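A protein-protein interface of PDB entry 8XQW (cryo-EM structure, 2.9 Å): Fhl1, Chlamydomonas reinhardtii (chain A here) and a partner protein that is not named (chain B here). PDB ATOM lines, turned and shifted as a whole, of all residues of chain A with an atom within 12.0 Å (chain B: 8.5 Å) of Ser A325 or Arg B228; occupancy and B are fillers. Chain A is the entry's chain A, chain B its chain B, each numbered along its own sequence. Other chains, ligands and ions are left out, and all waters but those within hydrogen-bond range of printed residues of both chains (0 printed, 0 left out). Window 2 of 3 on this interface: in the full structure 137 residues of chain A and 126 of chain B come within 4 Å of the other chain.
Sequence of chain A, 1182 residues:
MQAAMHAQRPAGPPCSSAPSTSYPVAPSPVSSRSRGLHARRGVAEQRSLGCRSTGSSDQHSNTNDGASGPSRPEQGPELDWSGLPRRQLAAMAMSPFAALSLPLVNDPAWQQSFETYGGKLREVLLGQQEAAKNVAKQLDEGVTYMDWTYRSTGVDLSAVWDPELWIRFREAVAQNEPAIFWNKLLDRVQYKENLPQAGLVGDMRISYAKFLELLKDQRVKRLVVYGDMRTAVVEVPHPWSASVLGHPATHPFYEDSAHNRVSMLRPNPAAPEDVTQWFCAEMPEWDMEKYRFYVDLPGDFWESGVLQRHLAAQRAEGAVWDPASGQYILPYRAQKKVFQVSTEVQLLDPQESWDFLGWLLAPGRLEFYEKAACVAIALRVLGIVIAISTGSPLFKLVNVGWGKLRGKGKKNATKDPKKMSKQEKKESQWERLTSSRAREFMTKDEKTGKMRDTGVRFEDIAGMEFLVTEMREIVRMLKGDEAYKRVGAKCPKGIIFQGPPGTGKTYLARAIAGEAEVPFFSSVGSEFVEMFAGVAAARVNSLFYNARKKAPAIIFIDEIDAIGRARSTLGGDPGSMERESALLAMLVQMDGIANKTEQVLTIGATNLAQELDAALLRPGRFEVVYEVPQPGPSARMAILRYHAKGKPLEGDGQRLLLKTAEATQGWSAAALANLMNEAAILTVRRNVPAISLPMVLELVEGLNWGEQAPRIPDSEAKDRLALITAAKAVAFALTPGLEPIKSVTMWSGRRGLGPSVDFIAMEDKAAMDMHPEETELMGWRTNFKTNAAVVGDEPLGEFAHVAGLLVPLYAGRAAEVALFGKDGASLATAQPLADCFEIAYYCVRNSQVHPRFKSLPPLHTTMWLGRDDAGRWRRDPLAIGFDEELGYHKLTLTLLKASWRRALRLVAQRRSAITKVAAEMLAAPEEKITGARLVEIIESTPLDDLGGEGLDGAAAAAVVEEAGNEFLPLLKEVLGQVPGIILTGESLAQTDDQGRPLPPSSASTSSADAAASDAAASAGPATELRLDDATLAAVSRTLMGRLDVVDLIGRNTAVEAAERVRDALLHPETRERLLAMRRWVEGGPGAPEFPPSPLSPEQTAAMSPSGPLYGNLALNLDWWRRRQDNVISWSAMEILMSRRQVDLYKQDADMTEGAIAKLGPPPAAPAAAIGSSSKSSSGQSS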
ATOM      1  N   ALA A 319     -12.985   3.174 -11.658  1.00  0.00           N
ATOM      2  CA  ALA A 319     -12.253   4.411 -11.460  1.00  0.00           C
ATOM      3  C   ALA A 319     -11.360   4.301 -10.235  1.00  0.00           C
ATOM      4  O   ALA A 319     -11.686   3.630  -9.255  1.00  0.00           O
ATOM      5  CB  ALA A 319     -13.215   5.584 -11.305  1.00  0.00           C
ATOM      6  N   VAL A 320     -10.212   4.970 -10.295  1.00  0.00           N
ATOM      7  CA  VAL A 320      -9.264   4.960  -9.192  1.00  0.00           C
ATOM      8  C   VAL A 320      -8.809   6.383  -8.924  1.00  0.00           C
ATOM      9  O   VAL A 320      -9.049   7.294  -9.721  1.00  0.00           O
ATOM     10  CB  VAL A 320      -8.046   4.059  -9.472  1.00  0.00           C
ATOM     11  CG1 VAL A 320      -8.460   2.608  -9.507  1.00  0.00           C
ATOM     12  CG2 VAL A 320      -7.398   4.458 -10.767  1.00  0.00           C
ATOM     13  N   TRP A 321      -8.161   6.573  -7.784  1.00  0.00           N
ATOM     14  CA  TRP A 321      -7.576   7.851  -7.419  1.00  0.00           C
ATOM     15  C   TRP A 321      -6.069   7.752  -7.587  1.00  0.00           C
ATOM     16  O   TRP A 321      -5.441   6.851  -7.026  1.00  0.00           O
ATOM     17  CB  TRP A 321      -7.929   8.228  -5.981  1.00  0.00           C
ATOM     18  CG  TRP A 321      -7.018   9.262  -5.420  1.00  0.00           C
ATOM     19  CD1 TRP A 321      -5.891   9.051  -4.688  1.00  0.00           C
ATOM     20  CD2 TRP A 321      -7.153  10.676  -5.553  1.00  0.00           C
ATOM     21  NE1 TRP A 321      -5.312  10.248  -4.359  1.00  0.00           N
ATOM     22  CE2 TRP A 321      -6.071  11.262  -4.880  1.00  0.00           C
ATOM     23  CE3 TRP A 321      -8.083  11.506  -6.180  1.00  0.00           C
ATOM     24  CZ2 TRP A 321      -5.893  12.635  -4.814  1.00  0.00           C
ATOM     25  CZ3 TRP A 321      -7.906  12.868  -6.111  1.00  0.00           C
ATOM     26  CH2 TRP A 321      -6.823  13.420  -5.432  1.00  0.00           C
ATOM     27  N   ASP A 322      -5.491   8.665  -8.358  1.00  0.00           N
ATOM     28  CA  ASP A 322      -4.045   8.712  -8.464  1.00  0.00           C
ATOM     29  C   ASP A 322      -3.527   9.893  -7.667  1.00  0.00           C
ATOM     30  O   ASP A 322      -3.876  11.043  -7.982  1.00  0.00           O
ATOM     31  CB  ASP A 322      -3.596   8.820  -9.913  1.00  0.00           C
ATOM     32  CG  ASP A 322      -2.102   8.989 -10.032  1.00  0.00           C
ATOM     33  OD1 ASP A 322      -1.373   8.030  -9.715  1.00  0.00           O
ATOM     34  OD2 ASP A 322      -1.653  10.082 -10.426  1.00  0.00           O
ATOM     35  N   PRO A 323      -2.720   9.669  -6.636  1.00  0.00           N
ATOM     36  CA  PRO A 323      -2.197  10.785  -5.845  1.00  0.00           C
ATOM     37  C   PRO A 323      -0.978  11.419  -6.486  1.00  0.00           C
ATOM     38  O   PRO A 323      -0.610  12.548  -6.157  1.00  0.00           O
ATOM     39  CB  PRO A 323      -1.851  10.121  -4.513  1.00  0.00           C
ATOM     40  CG  PRO A 323      -1.483   8.732  -4.896  1.00  0.00           C
ATOM     41  CD  PRO A 323      -2.340   8.364  -6.072  1.00  0.00           C
ATOM     42  N   ALA A 324      -0.332  10.689  -7.398  1.00  0.00           N
ATOM     43  CA  ALA A 324       0.805  11.256  -8.114  1.00  0.00           C
ATOM     44  C   ALA A 324       0.374  12.409  -9.003  1.00  0.00           C
ATOM     45  O   ALA A 324       1.161  13.324  -9.260  1.00  0.00           O
ATOM     46  CB  ALA A 324       1.500  10.178  -8.941  1.00  0.00           C
ATOM     47  N   SER A 325      -0.863  12.380  -9.485  1.00  0.00           N
ATOM     48  CA  SER A 325      -1.442  13.508 -10.188  1.00  0.00           C
ATOM     49  C   SER A 325      -2.612  14.129  -9.449  1.00  0.00           C
ATOM     50  O   SER A 325      -3.133  15.152  -9.901  1.00  0.00           O
ATOM     51  CB  SER A 325      -1.905  13.092 -11.591  1.00  0.00           C
ATOM     52  OG  SER A 325      -3.298  12.860 -11.603  1.00  0.00           O
ATOM     53  N   GLY A 326      -3.036  13.547  -8.332  1.00  0.00           N
ATOM     54  CA  GLY A 326      -4.148  14.073  -7.575  1.00  0.00           C
ATOM     55  C   GLY A 326      -5.417  14.140  -8.392  1.00  0.00           C
ATOM     56  O   GLY A 326      -6.095  15.170  -8.406  1.00  0.00           O
ATOM     57  N   GLN A 327      -5.755  13.051  -9.074  1.00  0.00           N
ATOM     58  CA  GLN A 327      -6.897  13.077  -9.974  1.00  0.00           C
ATOM     59  C   GLN A 327      -7.676  11.778  -9.862  1.00  0.00           C
ATOM     60  O   GLN A 327      -7.240  10.814  -9.233  1.00  0.00           O
ATOM     61  CB  GLN A 327      -6.458  13.301 -11.419  1.00  0.00           C
ATOM     62  CG  GLN A 327      -6.064  14.722 -11.736  1.00  0.00           C
ATOM     63  CD  GLN A 327      -6.610  15.182 -13.064  1.00  0.00           C
ATOM     64  OE1 GLN A 327      -7.558  15.960 -13.122  1.00  0.00           O
ATOM     65  NE2 GLN A 327      -6.016  14.696 -14.143  1.00  0.00           N
ATOM     66  N   TYR A 328      -8.850  11.775 -10.479  1.00  0.00           N
ATOM     67  CA  TYR A 328      -9.647  10.571 -10.638  1.00  0.00           C
ATOM     68  C   TYR A 328      -9.450  10.045 -12.049  1.00  0.00           C
ATOM     69  O   TYR A 328      -9.810  10.713 -13.022  1.00  0.00           O
ATOM     70  CB  TYR A 328     -11.123  10.848 -10.371  1.00  0.00           C
ATOM     71  CG  TYR A 328     -11.433  11.027  -8.914  1.00  0.00           C
ATOM     72  CD1 TYR A 328     -11.210  10.005  -8.012  1.00  0.00           C
ATOM     73  CD2 TYR A 328     -11.941  12.216  -8.438  1.00  0.00           C
ATOM     74  CE1 TYR A 328     -11.486  10.162  -6.680  1.00  0.00           C
ATOM     75  CE2 TYR A 328     -12.223  12.381  -7.106  1.00  0.00           C
ATOM     76  CZ  TYR A 328     -11.992  11.352  -6.230  1.00  0.00           C
ATOM     77  OH  TYR A 328     -12.274  11.516  -4.899  1.00  0.00           O
ATOM     78  N   ILE A 329      -8.881   8.853 -12.152  1.00  0.00           N
ATOM     79  CA  ILE A 329      -8.464   8.283 -13.423  1.00  0.00           C
ATOM     80  C   ILE A 329      -9.351   7.090 -13.730  1.00  0.00           C
ATOM     81  O   ILE A 329      -9.571   6.236 -12.865  1.00  0.00           O
ATOM     82  CB  ILE A 329      -6.987   7.857 -13.382  1.00  0.00           C
ATOM     83  CG1 ILE A 329      -6.086   9.066 -13.150  1.00  0.00           C
ATOM     84  CG2 ILE A 329      -6.604   7.149 -14.654  1.00  0.00           C
ATOM     85  CD1 ILE A 329      -5.766   9.832 -14.399  1.00  0.00           C
ATOM     86  N   LEU A 330      -9.861   7.031 -14.958  1.00  0.00           N
ATOM     87  CA  LEU A 330     -10.458   5.805 -15.463  1.00  0.00           C
ATOM     88  C   LEU A 330      -9.402   5.086 -16.284  1.00  0.00           C
ATOM     89  O   LEU A 330      -9.180   5.448 -17.445  1.00  0.00           O
ATOM     90  CB  LEU A 330     -11.694   6.092 -16.310  1.00  0.00           C
ATOM     91  CG  LEU A 330     -12.363   4.809 -16.783  1.00  0.00           C
ATOM     92  CD1 LEU A 330     -12.719   3.954 -15.599  1.00  0.00           C
ATOM     93  CD2 LEU A 330     -13.595   5.116 -17.591  1.00  0.00           C
ATOM     94  N   PRO A 331      -8.726   4.081 -15.736  1.00  0.00           N
ATOM     95  CA  PRO A 331      -7.555   3.521 -16.411  1.00  0.00           C
ATOM     96  C   PRO A 331      -7.900   2.937 -17.770  1.00  0.00           C
ATOM     97  O   PRO A 331      -9.041   2.577 -18.053  1.00  0.00           O
ATOM     98  CB  PRO A 331      -7.078   2.436 -15.443  1.00  0.00           C
ATOM     99  CG  PRO A 331      -8.260   2.118 -14.626  1.00  0.00           C
ATOM    100  CD  PRO A 331      -9.020   3.383 -14.481  1.00  0.00           C
ATOM    101  N   TYR B 210       1.218  16.443 -26.242  1.00  0.00           N
ATOM    102  CA  TYR B 210       0.520  17.401 -25.391  1.00  0.00           C
ATOM    103  C   TYR B 210       1.132  18.791 -25.498  1.00  0.00           C
ATOM    104  O   TYR B 210       0.410  19.794 -25.530  1.00  0.00           O
ATOM    105  CB  TYR B 210       0.533  16.936 -23.939  1.00  0.00           C
ATOM    106  CG  TYR B 210       0.046  18.005 -22.991  1.00  0.00           C
ATOM    107  CD1 TYR B 210      -1.297  18.336 -22.921  1.00  0.00           C
ATOM    108  CD2 TYR B 210       0.935  18.702 -22.187  1.00  0.00           C
ATOM    109  CE1 TYR B 210      -1.745  19.316 -22.064  1.00  0.00           C
ATOM    110  CE2 TYR B 210       0.496  19.684 -21.327  1.00  0.00           C
ATOM    111  CZ  TYR B 210      -0.843  19.987 -21.268  1.00  0.00           C
ATOM    112  OH  TYR B 210      -1.285  20.967 -20.412  1.00  0.00           O
ATOM    113  N   HIS B 222       5.997  25.511 -16.427  1.00  0.00           N
ATOM    114  CA  HIS B 222       5.126  24.394 -16.095  1.00  0.00           C
ATOM    115  C   HIS B 222       5.805  23.049 -16.241  1.00  0.00           C
ATOM    116  O   HIS B 222       5.078  22.066 -16.438  1.00  0.00           O
ATOM    117  CB  HIS B 222       3.877  24.445 -16.970  1.00  0.00           C
ATOM    118  CG  HIS B 222       3.011  25.637 -16.715  1.00  0.00           C
ATOM    119  ND1 HIS B 222       3.088  26.786 -17.469  1.00  0.00           N
ATOM    120  CD2 HIS B 222       2.038  25.850 -15.799  1.00  0.00           C
ATOM    121  CE1 HIS B 222       2.207  27.662 -17.021  1.00  0.00           C
ATOM    122  NE2 HIS B 222       1.557  27.119 -16.009  1.00  0.00           N
ATOM    123  N   ALA B 223       7.139  22.985 -16.172  1.00  0.00           N
ATOM    124  CA  ALA B 223       7.845  21.716 -16.317  1.00  0.00           C
ATOM    125  C   ALA B 223       7.399  20.677 -15.296  1.00  0.00           C
ATOM    126  O   ALA B 223       7.346  19.487 -15.623  1.00  0.00           O
ATOM    127  CB  ALA B 223       9.352  21.938 -16.208  1.00  0.00           C
ATOM    128  N   ALA B 224       7.080  21.091 -14.069  1.00  0.00           N
ATOM    129  CA  ALA B 224       6.516  20.175 -13.091  1.00  0.00           C
ATOM    130  C   ALA B 224       5.013  20.012 -13.242  1.00  0.00           C
ATOM    131  O   ALA B 224       4.477  18.958 -12.883  1.00  0.00           O
ATOM    132  CB  ALA B 224       6.834  20.648 -11.669  1.00  0.00           C
ATOM    133  N   HIS B 225       4.328  21.027 -13.761  1.00  0.00           N
ATOM    134  CA  HIS B 225       2.900  20.927 -14.025  1.00  0.00           C
ATOM    135  C   HIS B 225       2.624  19.984 -15.189  1.00  0.00           C
ATOM    136  O   HIS B 225       1.723  19.137 -15.123  1.00  0.00           O
ATOM    137  CB  HIS B 225       2.346  22.322 -14.311  1.00  0.00           C
ATOM    138  CG  HIS B 225       0.856  22.410 -14.252  1.00  0.00           C
ATOM    139  ND1 HIS B 225       0.126  21.945 -13.181  1.00  0.00           N
ATOM    140  CD2 HIS B 225      -0.040  22.921 -15.126  1.00  0.00           C
ATOM    141  CE1 HIS B 225      -1.158  22.160 -13.400  1.00  0.00           C
ATOM    142  NE2 HIS B 225      -1.286  22.752 -14.574  1.00  0.00           N
ATOM    143  N   VAL B 226       3.406  20.115 -16.262  1.00  0.00           N
ATOM    144  CA  VAL B 226       3.258  19.207 -17.389  1.00  0.00           C
ATOM    145  C   VAL B 226       3.586  17.777 -16.977  1.00  0.00           C
ATOM    146  O   VAL B 226       3.065  16.825 -17.564  1.00  0.00           O
ATOM    147  CB  VAL B 226       4.114  19.673 -18.581  1.00  0.00           C
ATOM    148  CG1 VAL B 226       5.579  19.370 -18.348  1.00  0.00           C
ATOM    149  CG2 VAL B 226       3.634  19.022 -19.861  1.00  0.00           C
ATOM    150  N   ALA B 227       4.423  17.588 -15.956  1.00  0.00           N
ATOM    151  CA  ALA B 227       4.628  16.236 -15.447  1.00  0.00           C
ATOM    152  C   ALA B 227       3.364  15.711 -14.782  1.00  0.00           C
ATOM    153  O   ALA B 227       2.977  14.555 -14.989  1.00  0.00           O
ATOM    154  CB  ALA B 227       5.805  16.205 -14.476  1.00  0.00           C
ATOM    155  N   ARG B 228       2.703  16.552 -13.986  1.00  0.00           N
ATOM    156  CA  ARG B 228       1.443  16.153 -13.373  1.00  0.00           C
ATOM    157  C   ARG B 228       0.401  15.802 -14.420  1.00  0.00           C
ATOM    158  O   ARG B 228      -0.397  14.882 -14.212  1.00  0.00           O
ATOM    159  CB  ARG B 228       0.930  17.269 -12.468  1.00  0.00           C
ATOM    160  CG  ARG B 228      -0.416  16.997 -11.831  1.00  0.00           C
ATOM    161  CD  ARG B 228      -0.919  18.224 -11.088  1.00  0.00           C
ATOM    162  NE  ARG B 228      -0.117  18.509  -9.904  1.00  0.00           N
ATOM    163  CZ  ARG B 228       0.786  19.484  -9.821  1.00  0.00           C
ATOM    164  NH1 ARG B 228       1.008  20.281 -10.858  1.00  0.00           N
ATOM    165  NH2 ARG B 228       1.466  19.658  -8.697  1.00  0.00           N
ATOM    166  N   VAL B 229       0.399  16.499 -15.557  1.00  0.00           N
ATOM    167  CA  VAL B 229      -0.623  16.217 -16.559  1.00  0.00           C
ATOM    168  C   VAL B 229      -0.252  14.998 -17.398  1.00  0.00           C
ATOM    169  O   VAL B 229      -1.126  14.222 -17.794  1.00  0.00           O
ATOM    170  CB  VAL B 229      -0.885  17.452 -17.441  1.00  0.00           C
ATOM    171  CG1 VAL B 229       0.222  17.637 -18.450  1.00  0.00           C
ATOM    172  CG2 VAL B 229      -2.207  17.297 -18.155  1.00  0.00           C
ATOM    173  N   VAL B 230       1.041  14.785 -17.665  1.00  0.00           N
ATOM    174  CA  VAL B 230       1.434  13.641 -18.479  1.00  0.00           C
ATOM    175  C   VAL B 230       1.287  12.352 -17.688  1.00  0.00           C
ATOM    176  O   VAL B 230       0.898  11.316 -18.237  1.00  0.00           O
ATOM    177  CB  VAL B 230       2.864  13.811 -19.022  1.00  0.00           C
ATOM    178  CG1 VAL B 230       3.874  13.799 -17.901  1.00  0.00           C
ATOM    179  CG2 VAL B 230       3.180  12.705 -20.001  1.00  0.00           C
ATOM    180  N   ARG B 231       1.586  12.389 -16.387  1.00  0.00           N
ATOM    181  CA  ARG B 231       1.367  11.211 -15.558  1.00  0.00           C
ATOM    182  C   ARG B 231      -0.104  10.833 -15.544  1.00  0.00           C
ATOM    183  O   ARG B 231      -0.451   9.647 -15.518  1.00  0.00           O
ATOM    184  CB  ARG B 231       1.882  11.466 -14.142  1.00  0.00           C
ATOM    185  CG  ARG B 231       1.113  10.755 -13.048  1.00  0.00           C
ATOM    186  CD  ARG B 231       1.503   9.299 -12.965  1.00  0.00           C
ATOM    187  NE  ARG B 231       0.861   8.650 -11.831  1.00  0.00           N
ATOM    188  CZ  ARG B 231       1.035   7.377 -11.502  1.00  0.00           C
ATOM    189  NH1 ARG B 231       1.835   6.603 -12.220  1.00  0.00           N
ATOM    190  NH2 ARG B 231       0.406   6.878 -10.450  1.00  0.00           N
ATOM    191  N   SER B 232      -0.985  11.830 -15.580  1.00  0.00           N
ATOM    192  CA  SER B 232      -2.413  11.546 -15.612  1.00  0.00           C
ATOM    193  C   SER B 232      -2.835  10.998 -16.966  1.00  0.00           C
ATOM    194  O   SER B 232      -3.615  10.042 -17.039  1.00  0.00           O
ATOM    195  CB  SER B 232      -3.203  12.807 -15.282  1.00  0.00           C
ATOM    196  OG  SER B 232      -4.444  12.812 -15.964  1.00  0.00           O
ATOM    197  N   ARG B 233      -2.341  11.589 -18.047  1.00  0.00           N
ATOM    198  CA  ARG B 233      -2.736  11.189 -19.389  1.00  0.00           C
ATOM    199  C   ARG B 233      -2.108   9.872 -19.825  1.00  0.00           C
ATOM    200  O   ARG B 233      -2.573   9.274 -20.800  1.00  0.00           O
ATOM    201  CB  ARG B 233      -2.377  12.292 -20.383  1.00  0.00           C
ATOM    202  CG  ARG B 233      -2.981  12.131 -21.757  1.00  0.00           C
ATOM    203  CD  ARG B 233      -2.806  13.393 -22.566  1.00  0.00           C
ATOM    204  NE  ARG B 233      -3.629  14.475 -22.037  1.00  0.00           N
ATOM    205  CZ  ARG B 233      -3.864  15.615 -22.676  1.00  0.00           C
ATOM    206  NH1 ARG B 233      -3.337  15.826 -23.874  1.00  0.00           N
ATOM    207  NH2 ARG B 233      -4.627  16.543 -22.117  1.00  0.00           N
ATOM    208  N   ALA B 234      -1.085   9.395 -19.126  1.00  0.00           N
ATOM    209  CA  ALA B 234      -0.428   8.151 -19.494  1.00  0.00           C
ATOM    210  C   ALA B 234      -1.119   6.917 -18.940  1.00  0.00           C
ATOM    211  O   ALA B 234      -0.760   5.804 -19.331  1.00  0.00           O
ATOM    212  CB  ALA B 234       1.027   8.164 -19.023  1.00  0.00           C
ATOM    213  N   LEU B 235      -2.093   7.080 -18.045  1.00  0.00           N
ATOM    214  CA  LEU B 235      -2.815   5.953 -17.474  1.00  0.00           C
ATOM    215  C   LEU B 235      -4.221   5.791 -18.014  1.00  0.00           C
ATOM    216  O   LEU B 235      -4.602   4.678 -18.370  1.00  0.00           O
ATOM    217  CB  LEU B 235      -2.904   6.085 -15.954  1.00  0.00           C
ATOM    218  CG  LEU B 235      -1.600   6.068 -15.173  1.00  0.00           C
ATOM    219  CD1 LEU B 235      -1.917   5.916 -13.707  1.00  0.00           C
ATOM    220  CD2 LEU B 235      -0.717   4.939 -15.653  1.00  0.00           C
ATOM    221  N   PRO B 238      -8.818  11.419 -17.257  1.00  0.00           N
ATOM    222  CA  PRO B 238      -9.230  12.043 -15.998  1.00  0.00           C
ATOM    223  C   PRO B 238     -10.736  12.228 -15.944  1.00  0.00           C
ATOM    224  O   PRO B 238     -11.383  12.494 -16.957  1.00  0.00           O
ATOM    225  CB  PRO B 238      -8.501  13.387 -16.015  1.00  0.00           C
ATOM    226  CG  PRO B 238      -8.245  13.651 -17.452  1.00  0.00           C
ATOM    227  CD  PRO B 238      -8.010  12.324 -18.085  1.00  0.00           C
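Of the printed residues of chain B, Asp A322 touches Arg B231.
Of chain B, only Arg B231 (3.3 Å) comes within 4 Å of Ala A324.
Of chain B, only Arg B228 (3.5 Å) and Ser B232 (3.7 Å) come within 4 Å of Ser A325.
Of the printed residues of chain B, Gln A327 touches Ser B232 and Pro B238.
Of the printed residues of chain B, Pro A331 touches Leu B235.
Ala B224 touches none of the printed residues of chain A.
No residue of chain A comes within 4 Å of His B225.
No residue of chain A comes within 4 Å of Ala B227.
Arg B228 touches just one residue of chain A: Ser A325 (3.5 Å).
No residue of chain A comes within 4 Å of Val B229.
Of chain A, only Ser A325, Gln A327 and Ile A329 come within 4 Å of Ser B232.
Printed residues of chain A within 4 Å of Leu B235: Pro A331 (3.7 Å).
Printed residues of chain A within 4 Å of Pro B238: Gln A327 and Tyr A328.
The nearest printed residue of chain A that does not touch Pro B238 is Ile A329 (4.4 Å).
The side-chain carboxylate (OD1) of Asp A322 lies within salt-bridge range of the guanidinium group (NE) of Arg B231 (3.1 Å).
The side-chain hydroxyl (OG) of Ser B232 lies within hydrogen-bond range of the side-chain amide nitrogen (NE2) of Gln A327 (3.1 Å).
Hydrophobic or aromatic side chains of chain A within 4 Å of the printed part of chain B: Ala A324 and Ile A329.
Of the 16 printed residues of chain B, 5 touch a printed residue of chain A.
Hydrophobic or aromatic side chains of chain B within 4 Å of the printed part of chain A: Pro B238.
Among the printed residues, Asp or Glu carboxylates within 4 Å of a Lys or Arg side-chain nitrogen of the other chain: Asp A322 with Arg B231.
CB of Ala A324 touches NE of Arg B231 (3.3 Å).
Arg B228 touches Ser A325 (O to CB, 3.5 Å).
Ser A325 touches Ser B232 (OG to CB, 3.7 Å).
Gln A327 touches Pro B238 (NE2 to CB, 3.4 Å).
Tyr A328 touches Pro B238.
CD1 of Ile A329 touches O of Ser B232 (3.4 Å).
Pro A331 touches Leu B235.
The backbone carbonyl oxygen (O) of Val A320 lies within hydrogen-bond range of the backbone NH (N) of Ile A329 (2.9 Å).
The side-chain carboxylate (OD2) of Asp A322 lies close to the backbone NH (N) of Ala A324, 3.4 Å away.
The side-chain carboxylate (OD2) of Asp A322 sits at hydrogen-bond distance from the backbone NH (N) of Ser A325.
The backbone NH of Asp A322 lies within hydrogen-bond range of the backbone carbonyl oxygen of Gln A327 (2.9 Å).
ND1 of His B225 lies within hydrogen-bond range of NH1 of Arg B228 (3.0 Å).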
